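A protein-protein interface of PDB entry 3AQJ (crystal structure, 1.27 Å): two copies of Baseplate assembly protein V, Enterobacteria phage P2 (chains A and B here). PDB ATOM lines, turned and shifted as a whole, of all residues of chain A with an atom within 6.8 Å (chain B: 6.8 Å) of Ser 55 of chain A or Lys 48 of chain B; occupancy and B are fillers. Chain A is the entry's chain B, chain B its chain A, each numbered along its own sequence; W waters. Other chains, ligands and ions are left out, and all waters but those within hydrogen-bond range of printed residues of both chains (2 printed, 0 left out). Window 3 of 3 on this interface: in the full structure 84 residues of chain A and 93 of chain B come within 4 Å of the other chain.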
ATOM      1  N   THR A  53      -7.953 -15.689  36.243  1.00  0.00           N
ATOM      2  CA  THR A  53      -7.010 -16.589  35.607  1.00  0.00           C
ATOM      3  C   THR A  53      -7.576 -16.996  34.271  1.00  0.00           C
ATOM      4  O   THR A  53      -8.750 -17.439  34.159  1.00  0.00           O
ATOM      5  CB  THR A  53      -6.731 -17.759  36.458  1.00  0.00           C
ATOM      6  OG1 THR A  53      -7.743 -18.865  36.531  1.00  0.00           O
ATOM      7  CG2 THR A  53      -6.325 -16.922  37.736  1.00  0.00           C
ATOM      8  N   ALA A  54      -6.792 -16.861  33.233  1.00  0.00           N
ATOM      9  CA  ALA A  54      -7.288 -17.017  31.872  1.00  0.00           C
ATOM     10  C   ALA A  54      -6.185 -17.688  31.044  1.00  0.00           C
ATOM     11  O   ALA A  54      -4.997 -17.531  31.358  1.00  0.00           O
ATOM     12  CB  ALA A  54      -7.680 -15.717  31.212  1.00  0.00           C
ATOM     13  N   SER A  55      -6.574 -18.389  29.983  1.00  0.00           N
ATOM     14  CA  SER A  55      -5.544 -19.024  29.141  1.00  0.00           C
ATOM     15  C   SER A  55      -5.147 -18.159  27.953  1.00  0.00           C
ATOM     16  O   SER A  55      -4.118 -18.484  27.291  1.00  0.00           O
ATOM     17  CB  SER A  55      -6.053 -20.388  28.700  1.00  0.00           C
ATOM     18  OG  SER A  55      -7.212 -20.190  27.866  1.00  0.00           O
ATOM     19  N   GLY A  56      -5.835 -17.131  27.587  1.00  0.00           N
ATOM     20  CA  GLY A  56      -5.643 -16.354  26.345  1.00  0.00           C
ATOM     21  C   GLY A  56      -5.172 -14.956  26.703  1.00  0.00           C
ATOM     22  O   GLY A  56      -3.979 -14.662  26.697  1.00  0.00           O
ATOM     23  N   SER A  57      -6.132 -14.069  27.002  1.00  0.00           N
ATOM     24  CA  SER A  57      -5.746 -12.643  27.244  1.00  0.00           C
ATOM     25  C   SER A  57      -6.760 -12.043  28.175  1.00  0.00           C
ATOM     26  O   SER A  57      -7.955 -12.447  28.207  1.00  0.00           O
ATOM     27  CB  SER A  57      -5.728 -11.852  25.921  1.00  0.00           C
ATOM     28  OG  SER A  57      -7.008 -11.854  25.298  1.00  0.00           O
ATOM     29  N   VAL A  58      -6.312 -10.997  28.835  1.00  0.00           N
ATOM     30  CA  VAL A  58      -7.182 -10.042  29.575  1.00  0.00           C
ATOM     31  C   VAL A  58      -6.986  -8.661  28.984  1.00  0.00           C
ATOM     32  O   VAL A  58      -5.794  -8.229  28.881  1.00  0.00           O
ATOM     33  CB  VAL A  58      -6.902 -10.098  31.050  1.00  0.00           C
ATOM     34  CG1 VAL A  58      -7.639  -8.901  31.901  1.00  0.00           C
ATOM     35  CG2 VAL A  58      -7.316 -11.436  31.612  1.00  0.00           C
ATOM     36  N   ASP B  29     -18.095 -24.975  29.974  1.00  0.00           N
ATOM     37  CA  ASP B  29     -16.744 -25.031  29.428  1.00  0.00           C
ATOM     38  C   ASP B  29     -15.707 -25.230  30.508  1.00  0.00           C
ATOM     39  O   ASP B  29     -14.511 -25.181  30.198  1.00  0.00           O
ATOM     40  CB  ASP B  29     -16.404 -23.758  28.644  1.00  0.00           C
ATOM     41  CG  ASP B  29     -16.399 -22.514  29.523  1.00  0.00           C
ATOM     42  OD1 ASP B  29     -16.942 -22.562  30.648  1.00  0.00           O
ATOM     43  OD2 ASP B  29     -15.848 -21.485  29.089  1.00  0.00           O
ATOM     44  N   ALA B  31     -15.225 -23.206  33.164  1.00  0.00           N
ATOM     45  CA  ALA B  31     -14.913 -21.965  33.900  1.00  0.00           C
ATOM     46  C   ALA B  31     -15.753 -21.768  35.104  1.00  0.00           C
ATOM     47  O   ALA B  31     -16.879 -22.331  35.224  1.00  0.00           O
ATOM     48  CB  ALA B  31     -15.115 -20.772  32.952  1.00  0.00           C
ATOM     49  N   GLY B  46     -10.453 -20.307  34.651  1.00  0.00           N
ATOM     50  CA  GLY B  46     -10.785 -21.273  33.640  1.00  0.00           C
ATOM     51  C   GLY B  46     -11.360 -20.632  32.406  1.00  0.00           C
ATOM     52  O   GLY B  46     -12.009 -21.332  31.642  1.00  0.00           O
ATOM     53  N   ILE B  47     -11.202 -19.352  32.221  1.00  0.00           N
ATOM     54  CA  ILE B  47     -11.703 -18.643  31.006  1.00  0.00           C
ATOM     55  C   ILE B  47     -10.601 -18.591  29.982  1.00  0.00           C
ATOM     56  O   ILE B  47      -9.406 -18.766  30.301  1.00  0.00           O
ATOM     57  CB  ILE B  47     -12.223 -17.236  31.375  1.00  0.00           C
ATOM     58  CG1 ILE B  47     -11.097 -16.301  31.749  1.00  0.00           C
ATOM     59  CG2 ILE B  47     -13.299 -17.367  32.485  1.00  0.00           C
ATOM     60  CD1 ILE B  47     -11.567 -14.842  32.099  1.00  0.00           C
ATOM     61  N   LYS B  48     -10.974 -18.278  28.751  1.00  0.00           N
ATOM     62  CA  LYS B  48      -9.979 -17.957  27.709  1.00  0.00           C
ATOM     63  C   LYS B  48      -9.660 -16.469  27.646  1.00  0.00           C
ATOM     64  O   LYS B  48      -8.482 -16.093  27.602  1.00  0.00           O
ATOM     65  CB  LYS B  48     -10.392 -18.477  26.324  1.00  0.00           C
ATOM     66  CG  LYS B  48     -10.357 -19.996  26.250  1.00  0.00           C
ATOM     67  CD  LYS B  48     -10.993 -20.613  24.982  1.00  0.00           C
ATOM     68  CE  LYS B  48     -10.327 -20.272  23.613  1.00  0.00           C
ATOM     69  NZ  LYS B  48      -8.883 -20.623  23.528  1.00  0.00           N
ATOM     70  N   THR B  49     -10.685 -15.664  27.660  1.00  0.00           N
ATOM     71  CA  THR B  49     -10.496 -14.209  27.610  1.00  0.00           C
ATOM     72  C   THR B  49     -11.382 -13.501  28.576  1.00  0.00           C
ATOM     73  O   THR B  49     -12.522 -13.926  28.827  1.00  0.00           O
ATOM     74  CB  THR B  49     -10.724 -13.622  26.218  1.00  0.00           C
ATOM     75  OG1 THR B  49     -12.052 -13.827  25.784  1.00  0.00           O
ATOM     76  CG2 THR B  49      -9.771 -14.229  25.142  1.00  0.00           C
ATOM     77  N   ALA B  50     -10.910 -12.331  29.005  1.00  0.00           N
ATOM     78  CA  ALA B  50     -11.765 -11.312  29.688  1.00  0.00           C
ATOM     79  C   ALA B  50     -11.527 -10.036  29.015  1.00  0.00           C
ATOM     80  O   ALA B  50     -10.384  -9.705  28.597  1.00  0.00           O
ATOM     81  CB  ALA B  50     -11.483 -11.160  31.128  1.00  0.00           C
HETATM   82  O   HOH W   1      -9.012 -10.138  26.047  1.00  0.00           O
HETATM   83  O   HOH W   2      -7.027 -19.094  25.059  1.00  0.00           O
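The backbone NH (N) of Gly 46 of chain B lies within hydrogen-bond range of the backbone carbonyl oxygen (O) of Thr 53 of chain A (3.4 Å). N of Ala 50 of chain B lies within hydrogen-bond range of O of Ser 57 of chain A, at 3.1 Å. O of Lys 48 of chain B is in hydrogen-bond range of N of Ser 57 of chain A (3.2 Å). The backbone carbonyl oxygen (O) of Lys 48 of chain B sits at hydrogen-bond distance from the backbone NH (N) of Gly 56 of chain A. O of Ile 47 of chain B lies within hydrogen-bond range of N of Ser 55 of chain A (2.9 Å).
Among the printed residues, merely in contact across the chains: Ser 57 of chain A with Thr 49 of chain B (3.1 Å), Ala 54 of chain A with Ile 47 of chain B (3.2 Å), Val 58 of chain A with Ala 50 of chain B (3.4 Å), Ser 55 of chain A with Lys 48 of chain B (3.5 Å), Thr 53 of chain A with Ile 47 of chain B (3.6 Å) and Ala 54 of chain A with Lys 48 of chain B (3.7 Å).
Ser 55 of chain A touches just these residues of chain B: Ile 47 and Lys 48. Lys 48 of chain B touches just these residues of chain A: Ala 54 (3.7 Å), Ser 55 (3.5 Å), Gly 56 (2.8 Å) and Ser 57 (3.2 Å). Printed residues of chain A within 4 Å of Ala 50 of chain B: Ser 57 (3.1 Å) and Val 58 (3.4 Å). Of the printed residues of chain A, Thr 49 of chain B touches Ser 57 (3.1 Å). Printed residues of chain A within 4 Å of Ile 47 of chain B: Thr 53 (3.6 Å), Ala 54 (3.2 Å) and Ser 55 (2.9 Å). Of the printed residues of chain A, Gly 46 of chain B touches Thr 53. Ala 31 of chain B touches none of the printed residues of chain A. The nearest residue of chain B that does not touch Ser 55 of chain A is Thr 49 of chain B (5.5 Å). The nearest residue of chain A that does not touch Lys 48 of chain B is Val 58 of chain A (5.7 Å). The nearest printed residue of chain B that does not touch Val 58 of chain A is Thr 49 of chain B (5.4 Å).
Of the 6 printed residues of chain A, 6 touch a printed residue of chain B. Along chain A the printed residues that touch a printed residue of chain B span positions 53 to 58. Among the printed residues, 11 pairs touch across the chains. Among the printed residues, no Asp or Glu carboxylate lies within 4 Å of a Lys or Arg side-chain nitrogen of the other chain.
No position is printed for both chains. Of the 11 pairs that touch across the chains among the printed residues, none has its exchanged pair printed and touching as well.
Water W1 lies within hydrogen-bond range of OG of Ser 57 of chain A and O of Ala 50 of chain B. Water W2 lies within hydrogen-bond range of the side-chain amino group (NZ) of Lys 48 of chain B (2.9 Å), the side-chain hydroxyl (OG) of Ser 55 of chain A (3.0 Å) and the backbone NH (N) of Gly 56 of chain A (3.4 Å).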
